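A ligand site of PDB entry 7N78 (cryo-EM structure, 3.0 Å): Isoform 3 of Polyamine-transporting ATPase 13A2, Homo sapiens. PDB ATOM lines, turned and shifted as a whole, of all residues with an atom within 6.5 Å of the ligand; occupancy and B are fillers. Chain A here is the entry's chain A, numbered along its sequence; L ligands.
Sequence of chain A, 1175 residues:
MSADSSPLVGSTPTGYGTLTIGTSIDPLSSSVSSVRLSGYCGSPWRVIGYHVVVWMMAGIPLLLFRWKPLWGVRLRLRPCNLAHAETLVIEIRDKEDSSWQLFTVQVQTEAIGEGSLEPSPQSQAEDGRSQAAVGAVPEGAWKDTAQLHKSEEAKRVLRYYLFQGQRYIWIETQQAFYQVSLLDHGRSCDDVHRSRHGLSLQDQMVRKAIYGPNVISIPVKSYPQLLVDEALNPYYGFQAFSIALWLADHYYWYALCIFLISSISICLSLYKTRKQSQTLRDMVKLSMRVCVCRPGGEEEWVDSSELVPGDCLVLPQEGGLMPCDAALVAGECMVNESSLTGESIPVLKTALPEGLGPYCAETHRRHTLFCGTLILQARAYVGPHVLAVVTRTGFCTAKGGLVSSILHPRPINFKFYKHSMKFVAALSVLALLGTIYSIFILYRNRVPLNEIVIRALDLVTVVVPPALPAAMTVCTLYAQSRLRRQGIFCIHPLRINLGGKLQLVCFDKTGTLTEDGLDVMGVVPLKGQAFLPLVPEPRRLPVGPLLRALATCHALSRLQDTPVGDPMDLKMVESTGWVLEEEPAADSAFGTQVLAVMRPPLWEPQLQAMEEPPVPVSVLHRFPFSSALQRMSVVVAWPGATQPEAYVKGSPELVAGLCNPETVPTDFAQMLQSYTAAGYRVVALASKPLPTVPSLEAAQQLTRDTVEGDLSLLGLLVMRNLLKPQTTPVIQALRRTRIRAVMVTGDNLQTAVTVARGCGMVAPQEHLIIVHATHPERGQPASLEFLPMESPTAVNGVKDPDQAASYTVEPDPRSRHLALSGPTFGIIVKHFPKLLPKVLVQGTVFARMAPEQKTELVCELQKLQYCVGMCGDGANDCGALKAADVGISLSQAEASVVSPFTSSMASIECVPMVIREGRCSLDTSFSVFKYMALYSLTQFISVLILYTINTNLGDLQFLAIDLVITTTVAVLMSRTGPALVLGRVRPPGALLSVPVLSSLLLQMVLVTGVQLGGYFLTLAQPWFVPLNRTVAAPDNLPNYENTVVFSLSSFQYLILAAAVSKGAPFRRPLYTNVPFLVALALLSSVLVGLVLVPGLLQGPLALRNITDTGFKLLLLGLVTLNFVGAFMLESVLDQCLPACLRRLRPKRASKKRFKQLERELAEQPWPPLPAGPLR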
ATOM      1  N   TRP A 246      -2.718   3.727   3.017  1.00  0.00           N
ATOM      2  CA  TRP A 246      -2.484   5.125   3.308  1.00  0.00           C
ATOM      3  C   TRP A 246      -2.482   5.384   4.808  1.00  0.00           C
ATOM      4  O   TRP A 246      -1.737   6.231   5.287  1.00  0.00           O
ATOM      5  CB  TRP A 246      -3.539   5.994   2.639  1.00  0.00           C
ATOM      6  CG  TRP A 246      -3.413   6.058   1.158  1.00  0.00           C
ATOM      7  CD1 TRP A 246      -2.335   5.759   0.419  1.00  0.00           C
ATOM      8  CD2 TRP A 246      -4.429   6.453   0.243  1.00  0.00           C
ATOM      9  NE1 TRP A 246      -2.597   5.937  -0.900  1.00  0.00           N
ATOM     10  CE2 TRP A 246      -3.884   6.374  -1.042  1.00  0.00           C
ATOM     11  CE3 TRP A 246      -5.754   6.875   0.380  1.00  0.00           C
ATOM     12  CZ2 TRP A 246      -4.617   6.687  -2.174  1.00  0.00           C
ATOM     13  CZ3 TRP A 246      -6.462   7.183  -0.737  1.00  0.00           C
ATOM     14  CH2 TRP A 246      -5.897   7.092  -1.993  1.00  0.00           C
ATOM     15  N   ASP A 249       0.709   4.534   5.964  1.00  0.00           N
ATOM     16  CA  ASP A 249       1.722   5.400   5.378  1.00  0.00           C
ATOM     17  C   ASP A 249       1.612   6.840   5.865  1.00  0.00           C
ATOM     18  O   ASP A 249       2.224   7.726   5.284  1.00  0.00           O
ATOM     19  CB  ASP A 249       1.620   5.373   3.854  1.00  0.00           C
ATOM     20  CG  ASP A 249       2.912   5.705   3.190  1.00  0.00           C
ATOM     21  OD1 ASP A 249       3.898   5.982   3.900  1.00  0.00           O
ATOM     22  OD2 ASP A 249       2.966   5.689   1.937  1.00  0.00           O
ATOM     23  N   HIS A 250       0.840   7.089   6.925  1.00  0.00           N
ATOM     24  CA  HIS A 250       0.632   8.413   7.468  1.00  0.00           C
ATOM     25  C   HIS A 250       0.128   9.369   6.395  1.00  0.00           C
ATOM     26  O   HIS A 250       0.676  10.457   6.191  1.00  0.00           O
ATOM     27  CB  HIS A 250       1.903   8.935   8.134  1.00  0.00           C
ATOM     28  CG  HIS A 250       2.617   7.904   8.949  1.00  0.00           C
ATOM     29  ND1 HIS A 250       2.023   7.258  10.007  1.00  0.00           N
ATOM     30  CD2 HIS A 250       3.874   7.399   8.855  1.00  0.00           C
ATOM     31  CE1 HIS A 250       2.884   6.399  10.536  1.00  0.00           C
ATOM     32  NE2 HIS A 250       4.008   6.474   9.853  1.00  0.00           N
ATOM     33  N   TYR A 251      -0.932   8.964   5.715  1.00  0.00           N
ATOM     34  CA  TYR A 251      -1.595   9.769   4.709  1.00  0.00           C
ATOM     35  C   TYR A 251      -3.071   9.905   5.072  1.00  0.00           C
ATOM     36  O   TYR A 251      -3.949   9.630   4.260  1.00  0.00           O
ATOM     37  CB  TYR A 251      -1.439   9.159   3.325  1.00  0.00           C
ATOM     38  CG  TYR A 251      -1.691  10.120   2.192  1.00  0.00           C
ATOM     39  CD1 TYR A 251      -1.151  11.387   2.192  1.00  0.00           C
ATOM     40  CD2 TYR A 251      -2.480   9.773   1.122  1.00  0.00           C
ATOM     41  CE1 TYR A 251      -1.393  12.249   1.171  1.00  0.00           C
ATOM     42  CE2 TYR A 251      -2.722  10.635   0.100  1.00  0.00           C
ATOM     43  CZ  TYR A 251      -2.177  11.869   0.127  1.00  0.00           C
ATOM     44  OH  TYR A 251      -2.422  12.736  -0.908  1.00  0.00           O
ATOM     45  N   TYR A 254      -6.275  12.260   2.855  1.00  0.00           N
ATOM     46  CA  TYR A 254      -6.900  11.745   1.653  1.00  0.00           C
ATOM     47  C   TYR A 254      -7.527  10.386   1.896  1.00  0.00           C
ATOM     48  O   TYR A 254      -8.542  10.045   1.279  1.00  0.00           O
ATOM     49  CB  TYR A 254      -5.892  11.665   0.514  1.00  0.00           C
ATOM     50  CG  TYR A 254      -6.505  11.550  -0.845  1.00  0.00           C
ATOM     51  CD1 TYR A 254      -7.417  12.472  -1.296  1.00  0.00           C
ATOM     52  CD2 TYR A 254      -6.154  10.509  -1.690  1.00  0.00           C
ATOM     53  CE1 TYR A 254      -7.973  12.356  -2.539  1.00  0.00           C
ATOM     54  CE2 TYR A 254      -6.710  10.392  -2.934  1.00  0.00           C
ATOM     55  CZ  TYR A 254      -7.620  11.318  -3.354  1.00  0.00           C
ATOM     56  OH  TYR A 254      -8.165  11.197  -4.616  1.00  0.00           O
ATOM     57  N   GLU A 451       9.755  -0.061   4.407  1.00  0.00           N
ATOM     58  CA  GLU A 451       9.441   1.105   3.584  1.00  0.00           C
ATOM     59  C   GLU A 451       9.537   0.770   2.105  1.00  0.00           C
ATOM     60  O   GLU A 451       8.847   1.380   1.294  1.00  0.00           O
ATOM     61  CB  GLU A 451      10.332   2.276   3.941  1.00  0.00           C
ATOM     62  CG  GLU A 451       9.750   3.152   5.040  1.00  0.00           C
ATOM     63  CD  GLU A 451       8.664   4.087   4.537  1.00  0.00           C
ATOM     64  OE1 GLU A 451       8.961   4.917   3.648  1.00  0.00           O
ATOM     65  OE2 GLU A 451       7.521   4.005   5.024  1.00  0.00           O
ATOM     66  N   ARG A 455       6.423   1.759  -0.206  1.00  0.00           N
ATOM     67  CA  ARG A 455       6.496   2.608  -1.385  1.00  0.00           C
ATOM     68  C   ARG A 455       6.048   1.864  -2.634  1.00  0.00           C
ATOM     69  O   ARG A 455       5.351   2.425  -3.490  1.00  0.00           O
ATOM     70  CB  ARG A 455       7.920   3.139  -1.568  1.00  0.00           C
ATOM     71  CG  ARG A 455       8.485   3.876  -0.372  1.00  0.00           C
ATOM     72  CD  ARG A 455       8.232   5.362  -0.422  1.00  0.00           C
ATOM     73  NE  ARG A 455       6.817   5.701  -0.320  1.00  0.00           N
ATOM     74  CZ  ARG A 455       6.184   5.950   0.805  1.00  0.00           C
ATOM     75  NH1 ARG A 455       6.830   5.905   1.952  1.00  0.00           N
ATOM     76  NH2 ARG A 455       4.896   6.244   0.793  1.00  0.00           N
ATOM     77  N   ASP A 458       2.401   1.703  -2.547  1.00  0.00           N
ATOM     78  CA  ASP A 458       1.816   3.027  -2.659  1.00  0.00           C
ATOM     79  C   ASP A 458       1.816   3.512  -4.097  1.00  0.00           C
ATOM     80  O   ASP A 458       0.944   4.277  -4.486  1.00  0.00           O
ATOM     81  CB  ASP A 458       2.577   4.000  -1.763  1.00  0.00           C
ATOM     82  CG  ASP A 458       2.000   5.377  -1.800  1.00  0.00           C
ATOM     83  OD1 ASP A 458       1.112   5.662  -0.974  1.00  0.00           O
ATOM     84  OD2 ASP A 458       2.466   6.186  -2.622  1.00  0.00           O
ATOM     85  N   THR A 461      -1.535   2.594  -5.680  1.00  0.00           N
ATOM     86  CA  THR A 461      -2.592   3.572  -5.453  1.00  0.00           C
ATOM     87  C   THR A 461      -2.325   4.852  -6.206  1.00  0.00           C
ATOM     88  O   THR A 461      -3.263   5.578  -6.538  1.00  0.00           O
ATOM     89  CB  THR A 461      -2.740   3.847  -3.973  1.00  0.00           C
ATOM     90  OG1 THR A 461      -1.621   4.578  -3.500  1.00  0.00           O
ATOM     91  CG2 THR A 461      -2.825   2.558  -3.191  1.00  0.00           C
ATOM     92  N   VAL A 462      -1.060   5.163  -6.490  1.00  0.00           N
ATOM     93  CA  VAL A 462      -0.725   6.348  -7.282  1.00  0.00           C
ATOM     94  C   VAL A 462      -1.258   6.210  -8.690  1.00  0.00           C
ATOM     95  O   VAL A 462      -1.974   7.069  -9.186  1.00  0.00           O
ATOM     96  CB  VAL A 462       0.792   6.602  -7.279  1.00  0.00           C
ATOM     97  CG1 VAL A 462       1.168   7.431  -8.446  1.00  0.00           C
ATOM     98  CG2 VAL A 462       1.230   7.245  -6.006  1.00  0.00           C
ATOM     99  N   VAL A 463      -0.918   5.111  -9.368  1.00  0.00           N
ATOM    100  CA  VAL A 463      -1.234   4.997 -10.791  1.00  0.00           C
ATOM    101  C   VAL A 463      -2.646   4.482 -11.032  1.00  0.00           C
ATOM    102  O   VAL A 463      -3.245   4.787 -12.061  1.00  0.00           O
ATOM    103  CB  VAL A 463      -0.193   4.114 -11.501  1.00  0.00           C
ATOM    104  CG1 VAL A 463      -0.317   2.704 -11.031  1.00  0.00           C
ATOM    105  CG2 VAL A 463      -0.357   4.191 -12.999  1.00  0.00           C
ATOM    106  N   PRO A 466      -7.813   5.636  -6.718  1.00  0.00           N
ATOM    107  CA  PRO A 466      -8.997   5.167  -5.994  1.00  0.00           C
ATOM    108  C   PRO A 466     -10.192   6.100  -6.099  1.00  0.00           C
ATOM    109  O   PRO A 466     -11.290   5.706  -5.699  1.00  0.00           O
ATOM    110  CB  PRO A 466      -8.502   5.064  -4.547  1.00  0.00           C
ATOM    111  CG  PRO A 466      -7.025   5.050  -4.635  1.00  0.00           C
ATOM    112  CD  PRO A 466      -6.688   5.892  -5.812  1.00  0.00           C
ATOM    113  N   TYR A 935      -3.819  12.373 -14.920  1.00  0.00           N
ATOM    114  CA  TYR A 935      -3.390  12.742 -13.580  1.00  0.00           C
ATOM    115  C   TYR A 935      -2.654  11.596 -12.899  1.00  0.00           C
ATOM    116  O   TYR A 935      -1.581  11.785 -12.329  1.00  0.00           O
ATOM    117  CB  TYR A 935      -4.601  13.176 -12.758  1.00  0.00           C
ATOM    118  CG  TYR A 935      -4.513  12.934 -11.280  1.00  0.00           C
ATOM    119  CD1 TYR A 935      -3.647  13.655 -10.482  1.00  0.00           C
ATOM    120  CD2 TYR A 935      -5.318  11.992 -10.677  1.00  0.00           C
ATOM    121  CE1 TYR A 935      -3.569  13.429  -9.133  1.00  0.00           C
ATOM    122  CE2 TYR A 935      -5.245  11.754  -9.323  1.00  0.00           C
ATOM    123  CZ  TYR A 935      -4.375  12.479  -8.571  1.00  0.00           C
ATOM    124  OH  TYR A 935      -4.320  12.230  -7.224  1.00  0.00           O
ATOM    125  N   GLN A 939       1.344  11.692 -12.017  1.00  0.00           N
ATOM    126  CA  GLN A 939       1.822  11.476 -10.663  1.00  0.00           C
ATOM    127  C   GLN A 939       2.686  10.229 -10.586  1.00  0.00           C
ATOM    128  O   GLN A 939       3.645  10.192  -9.825  1.00  0.00           O
ATOM    129  CB  GLN A 939       0.621  11.390  -9.729  1.00  0.00           C
ATOM    130  CG  GLN A 939       0.918  11.583  -8.276  1.00  0.00           C
ATOM    131  CD  GLN A 939      -0.337  11.699  -7.469  1.00  0.00           C
ATOM    132  OE1 GLN A 939      -1.419  11.519  -7.988  1.00  0.00           O
ATOM    133  NE2 GLN A 939      -0.207  12.032  -6.213  1.00  0.00           N
ATOM    134  N   ASN A 952      10.892  11.722  -2.667  1.00  0.00           N
ATOM    135  CA  ASN A 952       9.480  11.559  -2.955  1.00  0.00           C
ATOM    136  C   ASN A 952       8.825  12.934  -2.920  1.00  0.00           C
ATOM    137  O   ASN A 952       9.467  13.948  -2.645  1.00  0.00           O
ATOM    138  CB  ASN A 952       8.807  10.609  -1.976  1.00  0.00           C
ATOM    139  CG  ASN A 952       7.660   9.855  -2.594  1.00  0.00           C
ATOM    140  OD1 ASN A 952       7.524   9.812  -3.794  1.00  0.00           O
ATOM    141  ND2 ASN A 952       6.839   9.248  -1.758  1.00  0.00           N
ATOM    142  N   GLY A 954       6.214  13.892  -0.859  1.00  0.00           N
ATOM    143  CA  GLY A 954       5.922  14.343   0.476  1.00  0.00           C
ATOM    144  C   GLY A 954       4.435  14.406   0.750  1.00  0.00           C
ATOM    145  O   GLY A 954       3.607  14.509  -0.151  1.00  0.00           O
ATOM    146  N   ASP A 955       4.079  14.344   2.036  1.00  0.00           N
ATOM    147  CA  ASP A 955       2.676  14.233   2.418  1.00  0.00           C
ATOM    148  C   ASP A 955       1.859  15.417   1.944  1.00  0.00           C
ATOM    149  O   ASP A 955       0.755  15.238   1.423  1.00  0.00           O
ATOM    150  CB  ASP A 955       2.561  14.070   3.933  1.00  0.00           C
ATOM    151  CG  ASP A 955       2.749  12.638   4.382  1.00  0.00           C
ATOM    152  OD1 ASP A 955       2.313  11.737   3.643  1.00  0.00           O
ATOM    153  OD2 ASP A 955       3.337  12.399   5.458  1.00  0.00           O
ATOM    154  N   PHE A 958       1.689  15.760  -1.982  1.00  0.00           N
ATOM    155  CA  PHE A 958       0.730  14.739  -2.389  1.00  0.00           C
ATOM    156  C   PHE A 958      -0.688  15.171  -2.066  1.00  0.00           C
ATOM    157  O   PHE A 958      -1.596  14.970  -2.870  1.00  0.00           O
ATOM    158  CB  PHE A 958       1.050  13.425  -1.675  1.00  0.00           C
ATOM    159  CG  PHE A 958       1.942  12.519  -2.441  1.00  0.00           C
ATOM    160  CD1 PHE A 958       1.636  12.134  -3.709  1.00  0.00           C
ATOM    161  CD2 PHE A 958       3.083  12.019  -1.865  1.00  0.00           C
ATOM    162  CE1 PHE A 958       2.447  11.283  -4.407  1.00  0.00           C
ATOM    163  CE2 PHE A 958       3.912  11.180  -2.555  1.00  0.00           C
ATOM    164  CZ  PHE A 958       3.590  10.808  -3.831  1.00  0.00           C
ATOM    165  N   ASP A 962      -3.632  15.812  -4.735  1.00  0.00           N
ATOM    166  CA  ASP A 962      -4.732  14.856  -4.698  1.00  0.00           C
ATOM    167  C   ASP A 962      -6.050  15.522  -4.363  1.00  0.00           C
ATOM    168  O   ASP A 962      -7.068  15.217  -4.975  1.00  0.00           O
ATOM    169  CB  ASP A 962      -4.438  13.763  -3.679  1.00  0.00           C
ATOM    170  CG  ASP A 962      -3.386  12.786  -4.148  1.00  0.00           C
ATOM    171  OD1 ASP A 962      -2.843  12.972  -5.234  1.00  0.00           O
ATOM    172  OD2 ASP A 962      -3.112  11.821  -3.419  1.00  0.00           O
ATOM    173  N   ALA A1033      13.140  10.106   1.772  1.00  0.00           N
ATOM    174  CA  ALA A1033      12.072  11.047   2.058  1.00  0.00           C
ATOM    175  C   ALA A1033      11.178  10.507   3.177  1.00  0.00           C
ATOM    176  O   ALA A1033      11.064   9.284   3.354  1.00  0.00           O
ATOM    177  CB  ALA A1033      11.234  11.294   0.816  1.00  0.00           C
ATOM    178  N   PRO A1034      10.537  11.390   3.950  1.00  0.00           N
ATOM    179  CA  PRO A1034      10.574  12.847   3.859  1.00  0.00           C
ATOM    180  C   PRO A1034      11.702  13.483   4.650  1.00  0.00           C
ATOM    181  O   PRO A1034      11.618  14.644   5.011  1.00  0.00           O
ATOM    182  CB  PRO A1034       9.226  13.256   4.439  1.00  0.00           C
ATOM    183  CG  PRO A1034       8.985  12.252   5.487  1.00  0.00           C
ATOM    184  CD  PRO A1034       9.590  10.958   4.994  1.00  0.00           C
HETATM  185  N1  LIG L   1      -2.851   9.438  -4.229  1.00  0.00           N
HETATM  186  C1  LIG L   1      -1.556   8.760  -4.319  1.00  0.00           C
HETATM  187  C2  LIG L   1      -1.188   8.183  -2.955  1.00  0.00           C
HETATM  188  C3  LIG L   1       0.003   8.968  -2.413  1.00  0.00           C
HETATM  189  N2  LIG L   1       0.358   8.466  -1.083  1.00  0.00           N
HETATM  190  C4  LIG L   1       1.378   9.391  -0.585  1.00  0.00           C
HETATM  191  C5  LIG L   1       1.935   8.927   0.755  1.00  0.00           C
HETATM  192  C6  LIG L   1       3.133   9.803   1.102  1.00  0.00           C
HETATM  193  C7  LIG L   1       3.808   9.303   2.379  1.00  0.00           C
HETATM  194  N3  LIG L   1       5.053  10.031   2.599  1.00  0.00           N
HETATM  195  C8  LIG L   1       5.814   9.345   3.658  1.00  0.00           C
HETATM  196  C9  LIG L   1       5.321   9.794   5.034  1.00  0.00           C
HETATM  197  C10 LIG L   1       5.959   8.908   6.096  1.00  0.00           C
HETATM  198  N4  LIG L   1       5.883   9.565   7.400  1.00  0.00           N
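Trp 246 touches the ligand.
OD2 of Asp 249 touches C5 of the ligand, 3.6 Å away.
His 250 touches the ligand (CD2 to N4, 3.3 Å).
Tyr 251 touches the ligand.
NH2 of Arg 455 touches C7 of the ligand, 3.6 Å away.
Thr 461 touches the ligand (OG1 to C2, 3.7 Å).
Val 462 touches the ligand (CG2 to C1, 3.6 Å).
CD2 of Phe 958 touches C4 of the ligand (3.4 Å).
Hydrophobic or aromatic side chains within 4 Å of the ligand: Trp 246, His 250, Tyr 251, Val 462 and Phe 958.
The guanidinium group of Arg 455 lies within salt-bridge range of the side-chain carboxylate of Asp 249, 3.3 Å away.
The indole nitrogen of Trp 246 lies within hydrogen-bond range of the side-chain hydroxyl of Thr 461 (3.1 Å).
O of Asp 458 is in hydrogen-bond range of OG1 of Thr 461, 2.8 Å away.
N of Tyr 251 lies within hydrogen-bond range of O of Trp 246 (2.9 Å).
The side-chain carboxylate of Asp 962 lies within hydrogen-bond range of the side-chain amide nitrogen of Gln 939 (3.0 Å).
OH of Tyr 251 is in hydrogen-bond range of O of Phe 958 (3.1 Å).
OH of Tyr 935 is in hydrogen-bond range of OD1 of Asp 962 (2.6 Å).
OE1 of Glu 451 is in salt-bridge range of NH1 of Arg 455.
OD1 of Asp 955 lies within salt-bridge range of N3 of the ligand (3.4 Å).
OD1 of Asp 458 lies within salt-bridge range of N2 of the ligand (2.9 Å).
The side-chain carboxylate (OD2) of Asp 962 lies within salt-bridge range of a nitrogen (N1) of the ligand (2.5 Å).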
